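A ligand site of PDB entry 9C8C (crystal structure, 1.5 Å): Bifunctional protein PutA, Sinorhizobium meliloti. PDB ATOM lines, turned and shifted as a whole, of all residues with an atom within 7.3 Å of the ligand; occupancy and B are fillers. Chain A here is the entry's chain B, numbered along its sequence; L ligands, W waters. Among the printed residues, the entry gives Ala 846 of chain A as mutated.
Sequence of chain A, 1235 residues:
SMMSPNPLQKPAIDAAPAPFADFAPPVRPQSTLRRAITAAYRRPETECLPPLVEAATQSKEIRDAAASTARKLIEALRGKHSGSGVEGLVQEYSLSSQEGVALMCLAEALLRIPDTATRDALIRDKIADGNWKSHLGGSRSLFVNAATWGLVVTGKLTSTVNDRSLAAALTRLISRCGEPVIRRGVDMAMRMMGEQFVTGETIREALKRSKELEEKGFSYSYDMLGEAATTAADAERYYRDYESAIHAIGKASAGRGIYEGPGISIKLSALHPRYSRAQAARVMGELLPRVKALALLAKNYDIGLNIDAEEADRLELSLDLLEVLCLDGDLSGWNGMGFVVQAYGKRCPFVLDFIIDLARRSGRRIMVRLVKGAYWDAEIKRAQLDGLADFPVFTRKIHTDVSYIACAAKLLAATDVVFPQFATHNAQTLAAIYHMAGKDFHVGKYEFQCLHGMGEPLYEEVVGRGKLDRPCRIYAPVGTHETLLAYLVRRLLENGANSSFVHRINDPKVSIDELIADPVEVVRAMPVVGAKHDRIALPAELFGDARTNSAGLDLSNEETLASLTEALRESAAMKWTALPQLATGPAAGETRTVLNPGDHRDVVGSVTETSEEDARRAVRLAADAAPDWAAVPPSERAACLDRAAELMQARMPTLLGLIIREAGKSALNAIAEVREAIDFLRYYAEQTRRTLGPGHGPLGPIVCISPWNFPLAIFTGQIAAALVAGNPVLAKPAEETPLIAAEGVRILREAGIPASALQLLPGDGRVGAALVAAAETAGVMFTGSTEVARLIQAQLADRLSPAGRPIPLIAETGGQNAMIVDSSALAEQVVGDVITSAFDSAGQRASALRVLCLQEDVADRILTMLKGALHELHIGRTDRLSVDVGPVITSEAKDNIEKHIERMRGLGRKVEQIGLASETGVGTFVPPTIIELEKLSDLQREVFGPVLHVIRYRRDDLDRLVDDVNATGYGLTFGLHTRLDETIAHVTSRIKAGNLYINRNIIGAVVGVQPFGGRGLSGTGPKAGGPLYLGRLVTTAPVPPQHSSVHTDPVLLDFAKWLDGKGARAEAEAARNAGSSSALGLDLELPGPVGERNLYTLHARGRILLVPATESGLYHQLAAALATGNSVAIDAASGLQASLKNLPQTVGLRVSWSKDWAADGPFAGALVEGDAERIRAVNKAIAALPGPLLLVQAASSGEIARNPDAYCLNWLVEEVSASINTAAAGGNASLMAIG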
ATOM      1  N   ALA A 672     -24.208  26.009   6.438  1.00  0.00           N
ATOM      2  CA  ALA A 672     -24.005  24.929   7.392  1.00  0.00           C
ATOM      3  C   ALA A 672     -22.533  24.687   7.648  1.00  0.00           C
ATOM      4  O   ALA A 672     -22.160  24.306   8.766  1.00  0.00           O
ATOM      5  CB  ALA A 672     -24.682  23.649   6.894  1.00  0.00           C
ATOM      6  N   GLU A 676     -20.694  24.998  11.220  1.00  0.00           N
ATOM      7  CA  GLU A 676     -19.941  23.898  11.842  1.00  0.00           C
ATOM      8  C   GLU A 676     -18.567  24.367  12.293  1.00  0.00           C
ATOM      9  O   GLU A 676     -18.097  23.972  13.363  1.00  0.00           O
ATOM     10  CB  GLU A 676     -19.823  22.724  10.876  1.00  0.00           C
ATOM     11  CG  GLU A 676     -19.100  21.484  11.429  1.00  0.00           C
ATOM     12  CD  GLU A 676     -19.157  20.303  10.460  1.00  0.00           C
ATOM     13  OE1 GLU A 676     -20.276  19.948  10.026  1.00  0.00           O
ATOM     14  OE2 GLU A 676     -18.100  19.738  10.106  1.00  0.00           O
ATOM     15  N   PHE A 680     -17.332  24.063  16.078  1.00  0.00           N
ATOM     16  CA  PHE A 680     -16.081  23.444  16.520  1.00  0.00           C
ATOM     17  C   PHE A 680     -15.296  24.381  17.429  1.00  0.00           C
ATOM     18  O   PHE A 680     -14.767  23.962  18.471  1.00  0.00           O
ATOM     19  CB  PHE A 680     -15.202  23.074  15.314  1.00  0.00           C
ATOM     20  CG  PHE A 680     -15.539  21.754  14.665  1.00  0.00           C
ATOM     21  CD1 PHE A 680     -15.701  20.603  15.417  1.00  0.00           C
ATOM     22  CD2 PHE A 680     -15.637  21.672  13.285  1.00  0.00           C
ATOM     23  CE1 PHE A 680     -15.985  19.371  14.785  1.00  0.00           C
ATOM     24  CE2 PHE A 680     -15.904  20.462  12.641  1.00  0.00           C
ATOM     25  CZ  PHE A 680     -16.075  19.306  13.389  1.00  0.00           C
ATOM     26  N   PHE A 710     -14.975  19.622   3.081  1.00  0.00           N
ATOM     27  CA  PHE A 710     -15.363  20.557   4.128  1.00  0.00           C
ATOM     28  C   PHE A 710     -14.168  21.457   4.362  1.00  0.00           C
ATOM     29  O   PHE A 710     -13.492  21.387   5.398  1.00  0.00           O
ATOM     30  CB  PHE A 710     -15.808  19.839   5.402  1.00  0.00           C
ATOM     31  CG  PHE A 710     -17.125  19.176   5.251  1.00  0.00           C
ATOM     32  CD1 PHE A 710     -18.291  19.909   5.424  1.00  0.00           C
ATOM     33  CD2 PHE A 710     -17.212  17.844   4.885  1.00  0.00           C
ATOM     34  CE1 PHE A 710     -19.527  19.312   5.279  1.00  0.00           C
ATOM     35  CE2 PHE A 710     -18.441  17.235   4.738  1.00  0.00           C
ATOM     36  CZ  PHE A 710     -19.593  17.974   4.930  1.00  0.00           C
ATOM     37  N   ALA A 713     -14.777  23.756   7.558  1.00  0.00           N
ATOM     38  CA  ALA A 713     -15.228  23.205   8.828  1.00  0.00           C
ATOM     39  C   ALA A 713     -14.239  22.171   9.362  1.00  0.00           C
ATOM     40  O   ALA A 713     -13.835  22.232  10.524  1.00  0.00           O
ATOM     41  CB  ALA A 713     -16.628  22.581   8.683  1.00  0.00           C
ATOM     42  N   ILE A 714     -13.839  21.203   8.525  1.00  0.00           N
ATOM     43  CA  ILE A 714     -12.891  20.204   9.019  1.00  0.00           C
ATOM     44  C   ILE A 714     -11.508  20.818   9.195  1.00  0.00           C
ATOM     45  O   ILE A 714     -10.789  20.519  10.161  1.00  0.00           O
ATOM     46  CB  ILE A 714     -12.870  18.986   8.089  1.00  0.00           C
ATOM     47  CG1 ILE A 714     -14.189  18.234   8.241  1.00  0.00           C
ATOM     48  CG2 ILE A 714     -11.691  18.095   8.411  1.00  0.00           C
ATOM     49  CD1 ILE A 714     -14.278  17.067   7.271  1.00  0.00           C
ATOM     50  N   GLU A 812      -9.963  10.351  10.096  1.00  0.00           N
ATOM     51  CA  GLU A 812     -11.324  10.022   9.665  1.00  0.00           C
ATOM     52  C   GLU A 812     -11.300   9.770   8.173  1.00  0.00           C
ATOM     53  O   GLU A 812     -10.844  10.633   7.406  1.00  0.00           O
ATOM     54  CB  GLU A 812     -12.333  11.122  10.007  1.00  0.00           C
ATOM     55  CG  GLU A 812     -13.793  10.720   9.662  1.00  0.00           C
ATOM     56  CD  GLU A 812     -14.300  11.371   8.377  1.00  0.00           C
ATOM     57  OE1 GLU A 812     -14.685  12.557   8.420  1.00  0.00           O
ATOM     58  OE2 GLU A 812     -14.283  10.707   7.319  1.00  0.00           O
ATOM     59  N   ASP A 840     -27.102  15.677  -1.798  1.00  0.00           N
ATOM     60  CA  ASP A 840     -26.611  16.926  -1.236  1.00  0.00           C
ATOM     61  C   ASP A 840     -25.098  16.978  -1.366  1.00  0.00           C
ATOM     62  O   ASP A 840     -24.405  15.977  -1.153  1.00  0.00           O
ATOM     63  CB  ASP A 840     -27.055  17.039   0.239  1.00  0.00           C
ATOM     64  CG  ASP A 840     -26.511  18.272   0.941  1.00  0.00           C
ATOM     65  OD1 ASP A 840     -25.306  18.324   1.265  1.00  0.00           O
ATOM     66  OD2 ASP A 840     -27.324  19.185   1.223  1.00  0.00           O
ATOM     67  N   ARG A 845     -19.875  14.029   0.730  1.00  0.00           N
ATOM     68  CA  ARG A 845     -19.787  13.971   2.181  1.00  0.00           C
ATOM     69  C   ARG A 845     -19.283  12.594   2.587  1.00  0.00           C
ATOM     70  O   ARG A 845     -19.711  11.577   2.033  1.00  0.00           O
ATOM     71  CB  ARG A 845     -21.147  14.220   2.820  1.00  0.00           C
ATOM     72  CG  ARG A 845     -21.701  15.625   2.672  1.00  0.00           C
ATOM     73  CD  ARG A 845     -23.078  15.685   3.312  1.00  0.00           C
ATOM     74  NE  ARG A 845     -23.718  16.998   3.178  1.00  0.00           N
ATOM     75  CZ  ARG A 845     -23.730  17.918   4.135  1.00  0.00           C
ATOM     76  NH1 ARG A 845     -23.132  17.725   5.305  1.00  0.00           N
ATOM     77  NH2 ARG A 845     -24.360  19.070   3.918  1.00  0.00           N
ATOM     78  N   ALA A 846     -18.390  12.550   3.580  1.00  0.00           N
ATOM     79  CA  ALA A 846     -18.057  11.253   4.173  1.00  0.00           C
ATOM     80  C   ALA A 846     -19.305  10.518   4.661  1.00  0.00           C
ATOM     81  O   ALA A 846     -19.370   9.292   4.600  1.00  0.00           O
ATOM     82  CB  ALA A 846     -17.100  11.442   5.363  1.00  0.00           C
ATOM     83  N   SER A 847     -20.307  11.264   5.117  1.00  0.00           N
ATOM     84  CA  SER A 847     -21.550  10.754   5.683  1.00  0.00           C
ATOM     85  C   SER A 847     -22.589  10.364   4.622  1.00  0.00           C
ATOM     86  O   SER A 847     -23.638   9.825   4.993  1.00  0.00           O
ATOM     87  CB  SER A 847     -22.160  11.821   6.585  1.00  0.00           C
ATOM     88  OG  SER A 847     -22.344  13.021   5.826  1.00  0.00           O
ATOM     89  N   ALA A 848     -22.315  10.626   3.350  1.00  0.00           N
ATOM     90  CA  ALA A 848     -23.359  10.505   2.327  1.00  0.00           C
ATOM     91  C   ALA A 848     -23.905   9.086   2.236  1.00  0.00           C
ATOM     92  O   ALA A 848     -23.190   8.091   2.446  1.00  0.00           O
ATOM     93  CB  ALA A 848     -22.792  10.930   0.959  1.00  0.00           C
ATOM     94  N   THR A 973     -21.657   6.403   9.017  1.00  0.00           N
ATOM     95  CA  THR A 973     -23.061   6.732   9.266  1.00  0.00           C
ATOM     96  C   THR A 973     -23.958   5.573   8.830  1.00  0.00           C
ATOM     97  O   THR A 973     -23.581   4.735   7.996  1.00  0.00           O
ATOM     98  CB  THR A 973     -23.490   8.010   8.536  1.00  0.00           C
ATOM     99  OG1 THR A 973     -23.283   7.869   7.130  1.00  0.00           O
ATOM    100  CG2 THR A 973     -22.700   9.205   9.079  1.00  0.00           C
ATOM    101  N   ASN A 995     -22.313   6.663  13.840  1.00  0.00           N
ATOM    102  CA  ASN A 995     -23.368   7.674  13.817  1.00  0.00           C
ATOM    103  C   ASN A 995     -24.619   7.024  13.235  1.00  0.00           C
ATOM    104  O   ASN A 995     -24.690   6.771  12.036  1.00  0.00           O
ATOM    105  CB  ASN A 995     -22.952   8.904  13.009  1.00  0.00           C
ATOM    106  CG  ASN A 995     -22.029   9.820  13.798  1.00  0.00           C
ATOM    107  OD1 ASN A 995     -20.822   9.587  13.850  1.00  0.00           O
ATOM    108  ND2 ASN A 995     -22.593  10.835  14.425  1.00  0.00           N
ATOM    109  N   TYR A 997     -28.843   7.080  12.676  1.00  0.00           N
ATOM    110  CA  TYR A 997     -29.921   8.045  12.458  1.00  0.00           C
ATOM    111  C   TYR A 997     -31.210   7.286  12.241  1.00  0.00           C
ATOM    112  O   TYR A 997     -31.265   6.393  11.395  1.00  0.00           O
ATOM    113  CB  TYR A 997     -29.618   8.941  11.243  1.00  0.00           C
ATOM    114  CG  TYR A 997     -28.370   9.760  11.420  1.00  0.00           C
ATOM    115  CD1 TYR A 997     -28.395  10.958  12.129  1.00  0.00           C
ATOM    116  CD2 TYR A 997     -27.145   9.319  10.911  1.00  0.00           C
ATOM    117  CE1 TYR A 997     -27.255  11.737  12.296  1.00  0.00           C
ATOM    118  CE2 TYR A 997     -25.985  10.099  11.089  1.00  0.00           C
ATOM    119  CZ  TYR A 997     -26.059  11.286  11.786  1.00  0.00           C
ATOM    120  OH  TYR A 997     -24.936  12.068  11.967  1.00  0.00           O
ATOM    121  N   ILE A1002     -29.069  11.140   7.083  1.00  0.00           N
ATOM    122  CA  ILE A1002     -27.867  10.647   7.766  1.00  0.00           C
ATOM    123  C   ILE A1002     -26.691  11.599   7.612  1.00  0.00           C
ATOM    124  O   ILE A1002     -25.548  11.194   7.866  1.00  0.00           O
ATOM    125  CB  ILE A1002     -27.487   9.237   7.282  1.00  0.00           C
ATOM    126  CG1 ILE A1002     -27.040   9.203   5.811  1.00  0.00           C
ATOM    127  CG2 ILE A1002     -28.651   8.288   7.530  1.00  0.00           C
ATOM    128  CD1 ILE A1002     -26.419   7.863   5.416  1.00  0.00           C
ATOM    129  N   ILE A1003     -26.934  12.841   7.213  1.00  0.00           N
ATOM    130  CA  ILE A1003     -25.876  13.808   6.968  1.00  0.00           C
ATOM    131  C   ILE A1003     -26.007  14.981   7.938  1.00  0.00           C
ATOM    132  O   ILE A1003     -26.980  15.109   8.680  1.00  0.00           O
ATOM    133  CB  ILE A1003     -25.870  14.294   5.506  1.00  0.00           C
ATOM    134  CG1 ILE A1003     -27.185  15.010   5.130  1.00  0.00           C
ATOM    135  CG2 ILE A1003     -25.608  13.131   4.585  1.00  0.00           C
ATOM    136  CD1 ILE A1003     -27.032  15.853   3.847  1.00  0.00           C
ATOM    137  N   GLY A1004     -25.000  15.846   7.921  1.00  0.00           N
ATOM    138  CA  GLY A1004     -25.086  17.068   8.696  1.00  0.00           C
ATOM    139  C   GLY A1004     -25.016  16.860  10.192  1.00  0.00           C
ATOM    140  O   GLY A1004     -25.722  17.544  10.945  1.00  0.00           O
ATOM    141  N   ALA A1005     -24.190  15.911  10.650  1.00  0.00           N
ATOM    142  CA  ALA A1005     -23.943  15.769  12.086  1.00  0.00           C
ATOM    143  C   ALA A1005     -23.540  17.106  12.692  1.00  0.00           C
ATOM    144  O   ALA A1005     -22.778  17.882  12.101  1.00  0.00           O
ATOM    145  CB  ALA A1005     -22.851  14.739  12.329  1.00  0.00           C
ATOM    146  N   VAL A1006     -24.066  17.358  13.890  1.00  0.00           N
ATOM    147  CA  VAL A1006     -23.911  18.642  14.570  1.00  0.00           C
ATOM    148  C   VAL A1006     -22.934  18.485  15.729  1.00  0.00           C
ATOM    149  O   VAL A1006     -23.087  17.578  16.551  1.00  0.00           O
ATOM    150  CB  VAL A1006     -25.270  19.177  15.042  1.00  0.00           C
ATOM    151  CG1 VAL A1006     -25.101  20.408  15.957  1.00  0.00           C
ATOM    152  CG2 VAL A1006     -26.144  19.530  13.832  1.00  0.00           C
ATOM    153  N   VAL A1007     -21.960  19.395  15.798  1.00  0.00           N
ATOM    154  CA  VAL A1007     -20.941  19.366  16.849  1.00  0.00           C
ATOM    155  C   VAL A1007     -21.607  19.320  18.222  1.00  0.00           C
ATOM    156  O   VAL A1007     -22.535  20.082  18.516  1.00  0.00           O
ATOM    157  CB  VAL A1007     -20.032  20.596  16.720  1.00  0.00           C
ATOM    158  CG1 VAL A1007     -19.144  20.706  17.954  1.00  0.00           C
ATOM    159  CG2 VAL A1007     -19.180  20.512  15.456  1.00  0.00           C
ATOM    160  N   GLY A1008     -21.131  18.402  19.069  1.00  0.00           N
ATOM    161  CA  GLY A1008     -21.606  18.274  20.434  1.00  0.00           C
ATOM    162  C   GLY A1008     -23.007  17.733  20.590  1.00  0.00           C
ATOM    163  O   GLY A1008     -23.505  17.653  21.717  1.00  0.00           O
ATOM    164  N   GLN A1010     -24.488  15.336  17.670  1.00  0.00           N
ATOM    165  CA  GLN A1010     -24.080  14.051  17.120  1.00  0.00           C
ATOM    166  C   GLN A1010     -22.573  14.060  16.906  1.00  0.00           C
ATOM    167  O   GLN A1010     -22.090  14.257  15.779  1.00  0.00           O
ATOM    168  CB  GLN A1010     -24.789  13.717  15.795  1.00  0.00           C
ATOM    169  CG  GLN A1010     -26.320  13.747  15.851  1.00  0.00           C
ATOM    170  CD  GLN A1010     -26.896  15.091  15.428  1.00  0.00           C
ATOM    171  OE1 GLN A1010     -26.296  15.837  14.639  1.00  0.00           O
ATOM    172  NE2 GLN A1010     -28.079  15.403  15.946  1.00  0.00           N
ATOM    173  N   PRO A1011     -21.787  13.897  17.976  1.00  0.00           N
ATOM    174  CA  PRO A1011     -20.339  13.737  17.815  1.00  0.00           C
ATOM    175  C   PRO A1011     -20.059  12.743  16.691  1.00  0.00           C
ATOM    176  O   PRO A1011     -20.708  11.695  16.594  1.00  0.00           O
ATOM    177  CB  PRO A1011     -19.895  13.215  19.179  1.00  0.00           C
ATOM    178  CG  PRO A1011     -20.895  13.795  20.139  1.00  0.00           C
ATOM    179  CD  PRO A1011     -22.207  13.767  19.388  1.00  0.00           C
ATOM    180  N   PHE A1012     -19.114  13.087  15.817  1.00  0.00           N
ATOM    181  CA  PHE A1012     -19.039  12.470  14.497  1.00  0.00           C
ATOM    182  C   PHE A1012     -17.760  11.648  14.345  1.00  0.00           C
ATOM    183  O   PHE A1012     -16.650  12.168  14.523  1.00  0.00           O
ATOM    184  CB  PHE A1012     -19.108  13.545  13.413  1.00  0.00           C
ATOM    185  CG  PHE A1012     -19.143  12.988  12.010  1.00  0.00           C
ATOM    186  CD1 PHE A1012     -20.297  12.440  11.503  1.00  0.00           C
ATOM    187  CD2 PHE A1012     -18.019  13.046  11.200  1.00  0.00           C
ATOM    188  CE1 PHE A1012     -20.345  11.917  10.216  1.00  0.00           C
ATOM    189  CE2 PHE A1012     -18.039  12.541   9.909  1.00  0.00           C
ATOM    190  CZ  PHE A1012     -19.205  11.968   9.406  1.00  0.00           C
ATOM    191  N   GLY A1013     -17.907  10.396  13.957  1.00  0.00           N
ATOM    192  CA  GLY A1013     -16.798   9.543  13.627  1.00  0.00           C
ATOM    193  C   GLY A1013     -17.186   8.095  13.835  1.00  0.00           C
ATOM    194  O   GLY A1013     -18.111   7.772  14.560  1.00  0.00           O
ATOM    195  N   ALA A1024     -14.842  13.604  16.308  1.00  0.00           N
ATOM    196  CA  ALA A1024     -14.808  15.060  16.207  1.00  0.00           C
ATOM    197  C   ALA A1024     -16.068  15.652  16.815  1.00  0.00           C
ATOM    198  O   ALA A1024     -17.151  15.072  16.719  1.00  0.00           O
ATOM    199  CB  ALA A1024     -14.701  15.475  14.739  1.00  0.00           C
ATOM    200  N   GLY A1025     -15.926  16.796  17.475  1.00  0.00           N
ATOM    201  CA  GLY A1025     -17.095  17.390  18.062  1.00  0.00           C
ATOM    202  C   GLY A1025     -17.652  16.602  19.224  1.00  0.00           C
ATOM    203  O   GLY A1025     -18.821  16.743  19.564  1.00  0.00           O
HETATM  204  C1  LIG L   1     -21.753  15.733   8.097  1.00  0.00           C
HETATM  205  C2  LIG L   1     -21.007  17.101   8.472  1.00  0.00           C
HETATM  206  C3  LIG L   1     -19.710  16.378  10.449  1.00  0.00           C
HETATM  207  C4  LIG L   1     -19.081  16.801  11.798  1.00  0.00           C
HETATM  208  C5  LIG L   1     -19.774  17.387  12.792  1.00  0.00           C
HETATM  209  N1  LIG L   1     -20.815  17.285   9.964  1.00  0.00           N
HETATM  210  O1  LIG L   1     -22.104  14.869   9.005  1.00  0.00           O
HETATM  211  O2  LIG L   1     -22.021  15.506   6.842  1.00  0.00           O
HETATM  212  O   HOH W   1     -19.489  14.106   6.048  1.00  0.00           O
HETATM  213  O   HOH W   2     -17.735  17.749   8.330  1.00  0.00           O
HETATM  214  O   HOH W   3     -15.910  16.430  11.190  1.00  0.00           O
HETATM  215  O   HOH W   4     -23.788  12.494   9.558  1.00  0.00           O
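The backbone carbonyl oxygen (O) of Phe 1012 sits at hydrogen-bond distance from the backbone NH (N) of Ala 1024, 2.9 Å away.
The backbone carbonyl oxygen of Ser 847 is in hydrogen-bond range of the side-chain hydroxyl of Thr 973 (2.9 Å).
The guanidinium group (NE) of Arg 845 is in salt-bridge range of the side-chain carboxylate (OD1) of Asp 840, at 2.8 Å.
Merely in contact with the ligand: Phe 710 and Phe 1012.
Within 4 Å of the ligand: Glu 676, Phe 710, Arg 845, Ser 847, Gly 1004, Ala 1005 and Phe 1012.
The nearest printed residue that does not touch the ligand is Ile 1003 (4.05 Å).
A nitrogen (N1) of the ligand is in salt-bridge range of the side-chain carboxylate (OE1) of Glu 676 (2.7 Å).
The guanidinium group (NH1) of Arg 845 lies within salt-bridge range of an oxygen (O2) of the ligand.
O2 of the ligand lies within hydrogen-bond range of N of Gly 1004, at 3.2 Å.
The side-chain hydroxyl of Ser 847 is in hydrogen-bond range of an oxygen (O2) of the ligand (2.7 Å).
An oxygen (O1) of the ligand lies within hydrogen-bond range of the backbone NH (N) of Ala 1005 (2.9 Å).
O of Ala 1005 sits at hydrogen-bond distance from N1 of the ligand.
Water W4 lies within hydrogen-bond range of the side-chain hydroxyl of Tyr 997 (2.7 Å), the backbone carbonyl oxygen of Ile 1002 (2.8 Å) and an oxygen (O1) of the ligand (3.0 Å).
Water W1 lies within hydrogen-bond range of an oxygen (O2) of the ligand (3.0 Å), the side-chain hydroxyl (OG) of Ser 847 (3.1 Å) and the backbone NH (N) of Ala 846 (3.1 Å).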
